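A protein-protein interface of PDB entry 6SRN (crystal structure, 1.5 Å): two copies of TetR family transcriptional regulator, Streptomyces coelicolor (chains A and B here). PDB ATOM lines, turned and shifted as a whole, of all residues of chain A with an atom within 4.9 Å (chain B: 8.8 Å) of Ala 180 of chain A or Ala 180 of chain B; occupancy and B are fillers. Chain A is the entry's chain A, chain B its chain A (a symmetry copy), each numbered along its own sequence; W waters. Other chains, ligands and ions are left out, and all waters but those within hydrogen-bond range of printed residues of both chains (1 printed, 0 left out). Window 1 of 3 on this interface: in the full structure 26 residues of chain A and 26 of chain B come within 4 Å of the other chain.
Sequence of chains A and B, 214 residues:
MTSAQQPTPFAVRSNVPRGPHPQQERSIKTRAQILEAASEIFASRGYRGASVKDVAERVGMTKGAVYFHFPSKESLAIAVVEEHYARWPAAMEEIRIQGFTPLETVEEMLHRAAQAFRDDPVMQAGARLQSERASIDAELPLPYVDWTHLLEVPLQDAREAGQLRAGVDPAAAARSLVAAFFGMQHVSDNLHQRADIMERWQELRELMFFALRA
The side-chain hydroxyl of Ser 176 of chain A lies close to the backbone NH of Leu 204 of chain B (3.5 Å).
OG of Ser 176 of chain B lies close to N of Leu 204 of chain A (3.5 Å).
The side-chain sulfur (SD) of Met 208 of chain B lies close to the side-chain sulfur (SD) of Met 208 of chain A.
The side-chain hydroxyl (OG) of Ser 176 of chain B sits at hydrogen-bond distance from the backbone carbonyl oxygen (O) of Ala 172 of chain B (3.0 Å).
O of Phe 182 of chain B sits at hydrogen-bond distance from NE2 of Gln 185 of chain B, at 3.3 Å.
The backbone NH (N) of Trp 201 of chain B sits at hydrogen-bond distance from the side-chain sulfur (SD) of Met 184 of chain B.
Among the printed residues, pairs that only touch across the chains: Arg 175 of chain A with Arg 200 of chain B, Ser 176 of chain A with Leu 207 of chain B, Ala 179 of chain A with Gly 183 of chain B, Ala 179 of chain A with Met 184 of chain B, Ala 179 of chain A with Val 187 of chain B, Ala 180 of chain A with Ala 180 of chain B, Phe 182 of chain A with Phe 182 of chain B, Phe 182 of chain A with Gly 183 of chain B, Phe 182 of chain A with His 186 of chain B, Gly 183 of chain A with Ala 179 of chain B, Gly 183 of chain A with Phe 182 of chain B, Gly 183 of chain A with Gly 183 of chain B, Met 184 of chain A with Ala 179 of chain B, Leu 204 of chain A with Met 208 of chain B, Met 208 of chain A with Leu 204 of chain B and Met 208 of chain A with Leu 207 of chain B.
Printed residues of chain B within 4 Å of Arg 175 of chain A: Arg 200 (3.5 Å).
Of the printed residues of chain B, Ala 180 of chain A touches Ala 180 (3.9 Å).
Ala 173 of chain B touches none of the printed residues of chain A.
Of the printed residues of chain A, Ala 180 of chain B touches Ala 180 (3.9 Å).
Printed residues of chain A within 4 Å of Phe 182 of chain B: Phe 182 and Gly 183.
Of the printed residues of chain A, Gly 183 of chain B touches Ala 179 (3.4 Å), Phe 182 (3.9 Å) and Gly 183 (3.7 Å).
Of the printed residues of chain A, His 186 of chain B touches Phe 182.
The nearest residue of chain B that does not touch Ala 180 of chain A is Leu 204 of chain B (4.4 Å).
The nearest residue of chain A that does not touch Ala 180 of chain B is Leu 204 of chain A (4.4 Å).
The nearest printed residue of chain B that does not touch Met 184 of chain A is Ala 180 of chain B (5.1 Å).
Of the 24 printed residues of chain B, 12 touch a printed residue of chain A.
Of the 12 printed residues of chain A, 9 touch a printed residue of chain B.
Among the printed residues, no Asp or Glu carboxylate lies within 4 Å of a Lys or Arg side-chain nitrogen of the other chain.
Ser 176 of chain A touches Leu 204 of chain B, and with the chains exchanged Leu 204 of chain A touches Ser 176 of chain B.
Ala 179 of chain A touches Gly 183 of chain B, and with the chains exchanged Gly 183 of chain A touches Ala 179 of chain B.
Ala 179 of chain A touches Met 184 of chain B, and with the chains exchanged Met 184 of chain A touches Ala 179 of chain B.
Phe 182 of chain A touches Gly 183 of chain B, and with the chains exchanged Gly 183 of chain A touches Phe 182 of chain B.
Positions printed for both chains: 175, 176, 177, 178, 179, 180, 181, 182, 183, 184, 204 and 208.
Water W1 lies within hydrogen-bond range of O of Arg 200 of chain B and OG of Ser 176 of chain A.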
ATOM      1  N   ARG A 175      31.798  20.388  20.337  1.00  0.00           N
ATOM      2  CA  ARG A 175      31.404  21.651  19.724  1.00  0.00           C
ATOM      3  C   ARG A 175      29.981  22.062  20.039  1.00  0.00           C
ATOM      4  O   ARG A 175      29.707  23.230  20.348  1.00  0.00           O
ATOM      5  CB  ARG A 175      31.565  21.606  18.211  1.00  0.00           C
ATOM      6  CG  ARG A 175      32.998  21.615  17.710  1.00  0.00           C
ATOM      7  CD  ARG A 175      33.040  21.653  16.201  1.00  0.00           C
ATOM      8  NE  ARG A 175      32.496  20.484  15.510  1.00  0.00           N
ATOM      9  CZ  ARG A 175      33.219  19.436  15.102  1.00  0.00           C
ATOM     10  NH1 ARG A 175      34.513  19.329  15.411  1.00  0.00           N
ATOM     11  NH2 ARG A 175      32.618  18.484  14.451  1.00  0.00           N
ATOM     12  N   SER A 176      29.060  21.122  19.932  1.00  0.00           N
ATOM     13  CA  SER A 176      27.622  21.398  20.148  1.00  0.00           C
ATOM     14  C   SER A 176      27.382  21.849  21.588  1.00  0.00           C
ATOM     15  O   SER A 176      26.598  22.760  21.871  1.00  0.00           O
ATOM     16  CB  SER A 176      26.763  20.204  19.807  1.00  0.00           C
ATOM     17  OG  SER A 176      26.859  19.869  18.398  1.00  0.00           O
ATOM     18  N   LEU A 177      27.987  21.134  22.511  1.00  0.00           N
ATOM     19  CA  LEU A 177      27.837  21.466  23.933  1.00  0.00           C
ATOM     20  C   LEU A 177      28.373  22.862  24.261  1.00  0.00           C
ATOM     21  O   LEU A 177      27.753  23.690  24.949  1.00  0.00           O
ATOM     22  CB  LEU A 177      28.524  20.454  24.821  1.00  0.00           C
ATOM     23  CG  LEU A 177      27.725  19.174  25.061  1.00  0.00           C
ATOM     24  CD1 LEU A 177      28.689  18.121  25.629  1.00  0.00           C
ATOM     25  CD2 LEU A 177      26.500  19.369  25.935  1.00  0.00           C
ATOM     26  N   VAL A 178      29.544  23.164  23.739  1.00  0.00           N
ATOM     27  CA  VAL A 178      30.158  24.480  24.031  1.00  0.00           C
ATOM     28  C   VAL A 178      29.315  25.589  23.407  1.00  0.00           C
ATOM     29  O   VAL A 178      29.025  26.588  24.044  1.00  0.00           O
ATOM     30  CB  VAL A 178      31.632  24.537  23.593  1.00  0.00           C
ATOM     31  CG1 VAL A 178      32.195  25.979  23.582  1.00  0.00           C
ATOM     32  CG2 VAL A 178      32.474  23.610  24.457  1.00  0.00           C
ATOM     33  N   ALA A 179      28.926  25.422  22.147  1.00  0.00           N
ATOM     34  CA  ALA A 179      28.124  26.473  21.493  1.00  0.00           C
ATOM     35  C   ALA A 179      26.770  26.636  22.178  1.00  0.00           C
ATOM     36  O   ALA A 179      26.319  27.769  22.418  1.00  0.00           O
ATOM     37  CB  ALA A 179      27.901  26.143  20.041  1.00  0.00           C
ATOM     38  N   ALA A 180      26.114  25.528  22.501  1.00  0.00           N
ATOM     39  CA  ALA A 180      24.797  25.617  23.165  1.00  0.00           C
ATOM     40  C   ALA A 180      24.892  26.267  24.553  1.00  0.00           C
ATOM     41  O   ALA A 180      24.059  27.101  24.933  1.00  0.00           O
ATOM     42  CB  ALA A 180      24.197  24.286  23.263  1.00  0.00           C
ATOM     43  N   PHE A 181      25.873  25.823  25.334  1.00  0.00           N
ATOM     44  CA  PHE A 181      26.097  26.385  26.655  1.00  0.00           C
ATOM     45  C   PHE A 181      26.439  27.889  26.545  1.00  0.00           C
ATOM     46  O   PHE A 181      25.887  28.726  27.236  1.00  0.00           O
ATOM     47  CB  PHE A 181      27.210  25.626  27.396  1.00  0.00           C
ATOM     48  CG  PHE A 181      27.409  26.102  28.802  1.00  0.00           C
ATOM     49  CD1 PHE A 181      28.105  27.275  29.037  1.00  0.00           C
ATOM     50  CD2 PHE A 181      26.787  25.478  29.854  1.00  0.00           C
ATOM     51  CE1 PHE A 181      28.249  27.778  30.303  1.00  0.00           C
ATOM     52  CE2 PHE A 181      26.911  25.981  31.134  1.00  0.00           C
ATOM     53  CZ  PHE A 181      27.672  27.118  31.364  1.00  0.00           C
ATOM     54  N   PHE A 182      27.336  28.214  25.623  1.00  0.00           N
ATOM     55  CA  PHE A 182      27.652  29.594  25.383  1.00  0.00           C
ATOM     56  C   PHE A 182      26.383  30.424  25.125  1.00  0.00           C
ATOM     57  O   PHE A 182      26.178  31.511  25.658  1.00  0.00           O
ATOM     58  CB  PHE A 182      28.601  29.766  24.194  1.00  0.00           C
ATOM     59  CG  PHE A 182      28.666  31.202  23.791  1.00  0.00           C
ATOM     60  CD1 PHE A 182      29.336  32.147  24.550  1.00  0.00           C
ATOM     61  CD2 PHE A 182      27.925  31.652  22.698  1.00  0.00           C
ATOM     62  CE1 PHE A 182      29.249  33.498  24.230  1.00  0.00           C
ATOM     63  CE2 PHE A 182      27.857  32.976  22.378  1.00  0.00           C
ATOM     64  CZ  PHE A 182      28.519  33.932  23.148  1.00  0.00           C
ATOM     65  N   GLY A 183      25.535  29.909  24.244  1.00  0.00           N
ATOM     66  CA  GLY A 183      24.363  30.648  23.873  1.00  0.00           C
ATOM     67  C   GLY A 183      23.402  30.818  25.044  1.00  0.00           C
ATOM     68  O   GLY A 183      22.865  31.901  25.299  1.00  0.00           O
ATOM     69  N   MET A 184      23.213  29.730  25.797  1.00  0.00           N
ATOM     70  CA  MET A 184      22.343  29.752  26.983  1.00  0.00           C
ATOM     71  C   MET A 184      22.810  30.813  27.985  1.00  0.00           C
ATOM     72  O   MET A 184      21.999  31.630  28.466  1.00  0.00           O
ATOM     73  CB  MET A 184      22.300  28.360  27.587  1.00  0.00           C
ATOM     74  CG  MET A 184      21.513  28.227  28.834  1.00  0.00           C
ATOM     75  SD  MET A 184      22.349  28.807  30.328  1.00  0.00           S
ATOM     76  CE  MET A 184      23.872  27.885  30.367  1.00  0.00           C
ATOM     77  N   LEU A 204      17.969  23.000  28.996  1.00  0.00           N
ATOM     78  CA  LEU A 204      18.703  22.718  27.768  1.00  0.00           C
ATOM     79  C   LEU A 204      19.593  21.461  27.948  1.00  0.00           C
ATOM     80  O   LEU A 204      19.625  20.621  27.047  1.00  0.00           O
ATOM     81  CB  LEU A 204      19.593  23.939  27.426  1.00  0.00           C
ATOM     82  CG  LEU A 204      20.638  23.747  26.322  1.00  0.00           C
ATOM     83  CD1 LEU A 204      19.985  23.359  25.029  1.00  0.00           C
ATOM     84  CD2 LEU A 204      21.455  25.044  26.170  1.00  0.00           C
ATOM     85  N   MET A 208      20.176  17.955  25.785  1.00  0.00           N
ATOM     86  CA  MET A 208      21.464  17.593  25.192  1.00  0.00           C
ATOM     87  C   MET A 208      21.940  16.276  25.730  1.00  0.00           C
ATOM     88  O   MET A 208      22.399  15.453  24.953  1.00  0.00           O
ATOM     89  CB  MET A 208      22.493  18.675  25.463  1.00  0.00           C
ATOM     90  CG  MET A 208      21.986  19.976  24.905  1.00  0.00           C
ATOM     91  SD  MET A 208      22.254  20.106  23.155  1.00  0.00           S
ATOM     92  CE  MET A 208      24.063  20.144  22.937  1.00  0.00           C
ATOM     93  N   LEU B 110      14.519  26.958  11.431  1.00  0.00           N
ATOM     94  CA  LEU B 110      15.903  27.113  11.893  1.00  0.00           C
ATOM     95  C   LEU B 110      16.901  26.815  10.741  1.00  0.00           C
ATOM     96  O   LEU B 110      17.946  27.452  10.630  1.00  0.00           O
ATOM     97  CB  LEU B 110      16.184  26.281  13.164  1.00  0.00           C
ATOM     98  CG  LEU B 110      15.362  26.771  14.368  1.00  0.00           C
ATOM     99  CD1 LEU B 110      15.496  25.737  15.486  1.00  0.00           C
ATOM    100  CD2 LEU B 110      15.832  28.140  14.862  1.00  0.00           C
ATOM    101  N   TYR B 144      16.187  37.623  21.285  1.00  0.00           N
ATOM    102  CA  TYR B 144      15.775  36.234  21.620  1.00  0.00           C
ATOM    103  C   TYR B 144      14.271  36.055  21.803  1.00  0.00           C
ATOM    104  O   TYR B 144      13.730  34.973  21.468  1.00  0.00           O
ATOM    105  CB  TYR B 144      16.532  35.682  22.864  1.00  0.00           C
ATOM    106  CG  TYR B 144      18.008  36.030  22.835  1.00  0.00           C
ATOM    107  CD1 TYR B 144      18.840  35.656  21.766  1.00  0.00           C
ATOM    108  CD2 TYR B 144      18.581  36.810  23.842  1.00  0.00           C
ATOM    109  CE1 TYR B 144      20.147  36.056  21.724  1.00  0.00           C
ATOM    110  CE2 TYR B 144      19.902  37.186  23.798  1.00  0.00           C
ATOM    111  CZ  TYR B 144      20.678  36.837  22.720  1.00  0.00           C
ATOM    112  OH  TYR B 144      21.973  37.273  22.670  1.00  0.00           O
ATOM    113  N   ALA B 172       9.982  25.710  27.373  1.00  0.00           N
ATOM    114  CA  ALA B 172      11.366  25.391  27.648  1.00  0.00           C
ATOM    115  C   ALA B 172      12.112  24.964  26.405  1.00  0.00           C
ATOM    116  O   ALA B 172      13.250  25.358  26.215  1.00  0.00           O
ATOM    117  CB  ALA B 172      11.445  24.330  28.694  1.00  0.00           C
ATOM    118  N   ALA B 173      11.477  24.178  25.562  1.00  0.00           N
ATOM    119  CA  ALA B 173      12.055  23.755  24.295  1.00  0.00           C
ATOM    120  C   ALA B 173      12.315  24.947  23.380  1.00  0.00           C
ATOM    121  O   ALA B 173      13.355  24.990  22.722  1.00  0.00           O
ATOM    122  CB  ALA B 173      11.167  22.737  23.624  1.00  0.00           C
ATOM    123  N   ALA B 174      11.418  25.913  23.364  1.00  0.00           N
ATOM    124  CA  ALA B 174      11.572  27.078  22.524  1.00  0.00           C
ATOM    125  C   ALA B 174      12.789  27.853  23.046  1.00  0.00           C
ATOM    126  O   ALA B 174      13.624  28.279  22.271  1.00  0.00           O
ATOM    127  CB  ALA B 174      10.335  27.952  22.573  1.00  0.00           C
ATOM    128  N   ARG B 175      12.845  28.120  24.346  1.00  0.00           N
ATOM    129  CA  ARG B 175      14.017  28.803  24.883  1.00  0.00           C
ATOM    130  C   ARG B 175      15.322  28.098  24.579  1.00  0.00           C
ATOM    131  O   ARG B 175      16.316  28.732  24.200  1.00  0.00           O
ATOM    132  CB  ARG B 175      13.909  28.982  26.390  1.00  0.00           C
ATOM    133  CG  ARG B 175      12.891  30.009  26.851  1.00  0.00           C
ATOM    134  CD  ARG B 175      12.926  30.166  28.353  1.00  0.00           C
ATOM    135  NE  ARG B 175      12.534  28.994  29.135  1.00  0.00           N
ATOM    136  CZ  ARG B 175      11.299  28.762  29.592  1.00  0.00           C
ATOM    137  NH1 ARG B 175      10.280  29.555  29.257  1.00  0.00           N
ATOM    138  NH2 ARG B 175      11.098  27.705  30.321  1.00  0.00           N
ATOM    139  N   SER B 176      15.346  26.793  24.773  1.00  0.00           N
ATOM    140  CA  SER B 176      16.572  25.988  24.578  1.00  0.00           C
ATOM    141  C   SER B 176      17.018  26.051  23.118  1.00  0.00           C
ATOM    142  O   SER B 176      18.205  26.151  22.796  1.00  0.00           O
ATOM    143  CB  SER B 176      16.382  24.557  25.021  1.00  0.00           C
ATOM    144  OG  SER B 176      16.120  24.476  26.446  1.00  0.00           O
ATOM    145  N   LEU B 177      16.062  25.890  22.229  1.00  0.00           N
ATOM    146  CA  LEU B 177      16.362  25.931  20.792  1.00  0.00           C
ATOM    147  C   LEU B 177      16.925  27.286  20.357  1.00  0.00           C
ATOM    148  O   LEU B 177      17.926  27.412  19.632  1.00  0.00           O
ATOM    149  CB  LEU B 177      15.143  25.614  19.957  1.00  0.00           C
ATOM    150  CG  LEU B 177      14.834  24.123  19.824  1.00  0.00           C
ATOM    151  CD1 LEU B 177      13.396  23.989  19.303  1.00  0.00           C
ATOM    152  CD2 LEU B 177      15.833  23.362  18.972  1.00  0.00           C
ATOM    153  N   VAL B 178      16.298  28.345  20.827  1.00  0.00           N
ATOM    154  CA  VAL B 178      16.751  29.699  20.431  1.00  0.00           C
ATOM    155  C   VAL B 178      18.142  29.961  21.001  1.00  0.00           C
ATOM    156  O   VAL B 178      19.024  30.440  20.306  1.00  0.00           O
ATOM    157  CB  VAL B 178      15.734  30.784  20.824  1.00  0.00           C
ATOM    158  CG1 VAL B 178      16.319  32.215  20.723  1.00  0.00           C
ATOM    159  CG2 VAL B 178      14.462  30.637  20.001  1.00  0.00           C
ATOM    160  N   ALA B 179      18.343  29.657  22.279  1.00  0.00           N
ATOM    161  CA  ALA B 179      19.665  29.908  22.883  1.00  0.00           C
ATOM    162  C   ALA B 179      20.741  29.048  22.225  1.00  0.00           C
ATOM    163  O   ALA B 179      21.842  29.539  21.921  1.00  0.00           O
ATOM    164  CB  ALA B 179      19.639  29.614  24.359  1.00  0.00           C
ATOM    165  N   ALA B 180      20.445  27.774  21.994  1.00  0.00           N
ATOM    166  CA  ALA B 180      21.444  26.888  21.362  1.00  0.00           C
ATOM    167  C   ALA B 180      21.785  27.329  19.931  1.00  0.00           C
ATOM    168  O   ALA B 180      22.952  27.332  19.519  1.00  0.00           O
ATOM    169  CB  ALA B 180      20.959  25.507  21.369  1.00  0.00           C
ATOM    170  N   PHE B 181      20.747  27.632  19.156  1.00  0.00           N
ATOM    171  CA  PHE B 181      20.936  28.103  17.794  1.00  0.00           C
ATOM    172  C   PHE B 181      21.726  29.431  17.794  1.00  0.00           C
ATOM    173  O   PHE B 181      22.684  29.611  17.064  1.00  0.00           O
ATOM    174  CB  PHE B 181      19.587  28.271  17.077  1.00  0.00           C
ATOM    175  CG  PHE B 181      19.733  28.659  15.637  1.00  0.00           C
ATOM    176  CD1 PHE B 181      20.030  29.969  15.305  1.00  0.00           C
ATOM    177  CD2 PHE B 181      19.726  27.708  14.646  1.00  0.00           C
ATOM    178  CE1 PHE B 181      20.237  30.346  14.005  1.00  0.00           C
ATOM    179  CE2 PHE B 181      19.948  28.071  13.333  1.00  0.00           C
ATOM    180  CZ  PHE B 181      20.173  29.401  13.006  1.00  0.00           C
ATOM    181  N   PHE B 182      21.325  30.346  18.668  1.00  0.00           N
ATOM    182  CA  PHE B 182      22.052  31.576  18.806  1.00  0.00           C
ATOM    183  C   PHE B 182      23.550  31.320  19.041  1.00  0.00           C
ATOM    184  O   PHE B 182      24.433  31.927  18.443  1.00  0.00           O
ATOM    185  CB  PHE B 182      21.515  32.434  19.956  1.00  0.00           C
ATOM    186  CG  PHE B 182      22.467  33.543  20.259  1.00  0.00           C
ATOM    187  CD1 PHE B 182      22.611  34.635  19.420  1.00  0.00           C
ATOM    188  CD2 PHE B 182      23.343  33.431  21.339  1.00  0.00           C
ATOM    189  CE1 PHE B 182      23.614  35.572  19.651  1.00  0.00           C
ATOM    190  CE2 PHE B 182      24.313  34.362  21.571  1.00  0.00           C
ATOM    191  CZ  PHE B 182      24.470  35.456  20.722  1.00  0.00           C
ATOM    192  N   GLY B 183      23.834  30.423  19.978  1.00  0.00           N
ATOM    193  CA  GLY B 183      25.202  30.175  20.330  1.00  0.00           C
ATOM    194  C   GLY B 183      25.985  29.557  19.176  1.00  0.00           C
ATOM    195  O   GLY B 183      27.112  29.953  18.864  1.00  0.00           O
ATOM    196  N   MET B 184      25.352  28.590  18.503  1.00  0.00           N
ATOM    197  CA  MET B 184      25.966  27.929  17.342  1.00  0.00           C
ATOM    198  C   MET B 184      26.331  28.949  16.259  1.00  0.00           C
ATOM    199  O   MET B 184      27.468  28.948  15.746  1.00  0.00           O
ATOM    200  CB  MET B 184      25.023  26.853  16.835  1.00  0.00           C
ATOM    201  CG  MET B 184      25.468  26.132  15.620  1.00  0.00           C
ATOM    202  SD  MET B 184      25.222  27.025  14.069  1.00  0.00           S
ATOM    203  CE  MET B 184      23.482  27.406  14.052  1.00  0.00           C
ATOM    204  N   GLN B 185      25.383  29.830  15.945  1.00  0.00           N
ATOM    205  CA  GLN B 185      25.646  30.767  14.844  1.00  0.00           C
ATOM    206  C   GLN B 185      26.705  31.790  15.256  1.00  0.00           C
ATOM    207  O   GLN B 185      27.472  32.244  14.430  1.00  0.00           O
ATOM    208  CB  GLN B 185      24.367  31.371  14.293  1.00  0.00           C
ATOM    209  CG  GLN B 185      23.648  32.363  15.216  1.00  0.00           C
ATOM    210  CD  GLN B 185      24.301  33.736  15.192  1.00  0.00           C
ATOM    211  OE1 GLN B 185      24.822  34.192  14.191  1.00  0.00           O
ATOM    212  NE2 GLN B 185      24.258  34.414  16.318  1.00  0.00           N
ATOM    213  N   HIS B 186      26.706  32.175  16.535  1.00  0.00           N
ATOM    214  CA  HIS B 186      27.671  33.132  17.049  1.00  0.00           C
ATOM    215  C   HIS B 186      29.071  32.568  17.028  1.00  0.00           C
ATOM    216  O   HIS B 186      30.009  33.244  16.620  1.00  0.00           O
ATOM    217  CB  HIS B 186      27.268  33.570  18.443  1.00  0.00           C
ATOM    218  CG  HIS B 186      27.996  34.757  18.901  1.00  0.00           C
ATOM    219  ND1 HIS B 186      27.664  36.030  18.494  1.00  0.00           N
ATOM    220  CD2 HIS B 186      29.043  34.888  19.745  1.00  0.00           C
ATOM    221  CE1 HIS B 186      28.501  36.887  19.051  1.00  0.00           C
ATOM    222  NE2 HIS B 186      29.312  36.219  19.847  1.00  0.00           N
ATOM    223  N   VAL B 187      29.208  31.314  17.480  1.00  0.00           N
ATOM    224  CA  VAL B 187      30.504  30.696  17.412  1.00  0.00           C
ATOM    225  C   VAL B 187      30.994  30.619  15.966  1.00  0.00           C
ATOM    226  O   VAL B 187      32.159  30.886  15.688  1.00  0.00           O
ATOM    227  CB  VAL B 187      30.496  29.271  18.054  1.00  0.00           C
ATOM    228  CG1 VAL B 187      31.768  28.480  17.726  1.00  0.00           C
ATOM    229  CG2 VAL B 187      30.219  29.313  19.557  1.00  0.00           C
ATOM    230  N   ARG B 200      27.719  23.021  11.449  1.00  0.00           N
ATOM    231  CA  ARG B 200      27.654  23.202  12.904  1.00  0.00           C
ATOM    232  C   ARG B 200      26.208  23.054  13.353  1.00  0.00           C
ATOM    233  O   ARG B 200      25.926  22.478  14.410  1.00  0.00           O
ATOM    234  CB  ARG B 200      28.244  24.563  13.286  1.00  0.00           C
ATOM    235  CG  ARG B 200      29.704  24.789  12.904  1.00  0.00           C
ATOM    236  CD  ARG B 200      30.697  23.952  13.701  1.00  0.00           C
ATOM    237  NE  ARG B 200      30.719  22.555  13.311  1.00  0.00           N
ATOM    238  CZ  ARG B 200      31.317  22.090  12.219  1.00  0.00           C
ATOM    239  NH1 ARG B 200      32.009  22.894  11.388  1.00  0.00           N
ATOM    240  NH2 ARG B 200      31.237  20.803  11.962  1.00  0.00           N
ATOM    241  N   TRP B 201      25.270  23.624  12.603  1.00  0.00           N
ATOM    242  CA  TRP B 201      23.841  23.461  12.929  1.00  0.00           C
ATOM    243  C   TRP B 201      23.390  22.010  12.795  1.00  0.00           C
ATOM    244  O   TRP B 201      22.741  21.525  13.669  1.00  0.00           O
ATOM    245  CB  TRP B 201      22.976  24.419  12.114  1.00  0.00           C
ATOM    246  CG  TRP B 201      21.518  24.284  12.442  1.00  0.00           C
ATOM    247  CD1 TRP B 201      20.521  24.057  11.537  1.00  0.00           C
ATOM    248  CD2 TRP B 201      20.904  24.274  13.753  1.00  0.00           C
ATOM    249  NE1 TRP B 201      19.331  23.957  12.199  1.00  0.00           N
ATOM    250  CE2 TRP B 201      19.523  24.068  13.548  1.00  0.00           C
ATOM    251  CE3 TRP B 201      21.381  24.437  15.055  1.00  0.00           C
ATOM    252  CZ2 TRP B 201      18.608  24.002  14.607  1.00  0.00           C
ATOM    253  CZ3 TRP B 201      20.486  24.341  16.119  1.00  0.00           C
ATOM    254  CH2 TRP B 201      19.102  24.152  15.873  1.00  0.00           C
ATOM    255  N   LEU B 204      24.434  19.906  15.905  1.00  0.00           N
ATOM    256  CA  LEU B 204      23.741  20.290  17.129  1.00  0.00           C
ATOM    257  C   LEU B 204      22.226  19.983  17.009  1.00  0.00           C
ATOM    258  O   LEU B 204      21.648  19.458  17.964  1.00  0.00           O
ATOM    259  CB  LEU B 204      23.946  21.807  17.363  1.00  0.00           C
ATOM    260  CG  LEU B 204      23.085  22.462  18.450  1.00  0.00           C
ATOM    261  CD1 LEU B 204      23.326  21.818  19.783  1.00  0.00           C
ATOM    262  CD2 LEU B 204      23.390  23.971  18.492  1.00  0.00           C
ATOM    263  N   ARG B 205      21.609  20.328  15.893  1.00  0.00           N
ATOM    264  CA  ARG B 205      20.191  20.046  15.594  1.00  0.00           C
ATOM    265  C   ARG B 205      19.914  18.553  15.723  1.00  0.00           C
ATOM    266  O   ARG B 205      18.866  18.133  16.277  1.00  0.00           O
ATOM    267  CB  ARG B 205      19.978  20.529  14.182  1.00  0.00           C
ATOM    268  CG  ARG B 205      18.711  20.392  13.430  1.00  0.00           C
ATOM    269  CD  ARG B 205      19.223  20.626  12.014  1.00  0.00           C
ATOM    270  NE  ARG B 205      19.147  19.421  11.230  1.00  0.00           N
ATOM    271  CZ  ARG B 205      18.002  18.850  10.902  1.00  0.00           C
ATOM    272  NH1 ARG B 205      16.840  19.369  11.317  1.00  0.00           N
ATOM    273  NH2 ARG B 205      18.009  17.771  10.159  1.00  0.00           N
ATOM    274  N   LEU B 207      21.200  16.415  17.738  1.00  0.00           N
ATOM    275  CA  LEU B 207      21.010  16.132  19.157  1.00  0.00           C
ATOM    276  C   LEU B 207      19.705  16.731  19.692  1.00  0.00           C
ATOM    277  O   LEU B 207      18.929  16.065  20.372  1.00  0.00           O
ATOM    278  CB  LEU B 207      22.159  16.724  19.965  1.00  0.00           C
ATOM    279  CG  LEU B 207      23.568  16.246  19.652  1.00  0.00           C
ATOM    280  CD1 LEU B 207      24.574  17.030  20.483  1.00  0.00           C
ATOM    281  CD2 LEU B 207      23.708  14.764  19.910  1.00  0.00           C
ATOM    282  N   MET B 208      19.447  17.997  19.386  1.00  0.00           N
ATOM    283  CA  MET B 208      18.280  18.662  19.967  1.00  0.00           C
ATOM    284  C   MET B 208      17.014  18.003  19.506  1.00  0.00           C
ATOM    285  O   MET B 208      16.137  17.776  20.325  1.00  0.00           O
ATOM    286  CB  MET B 208      18.272  20.134  19.597  1.00  0.00           C
ATOM    287  CG  MET B 208      19.551  20.762  20.080  1.00  0.00           C
ATOM    288  SD  MET B 208      19.493  21.158  21.809  1.00  0.00           S
ATOM    289  CE  MET B 208      18.213  22.445  21.976  1.00  0.00           C
HETATM  290  O   HOH W   1      27.867  22.394  16.581  1.00  0.00           O
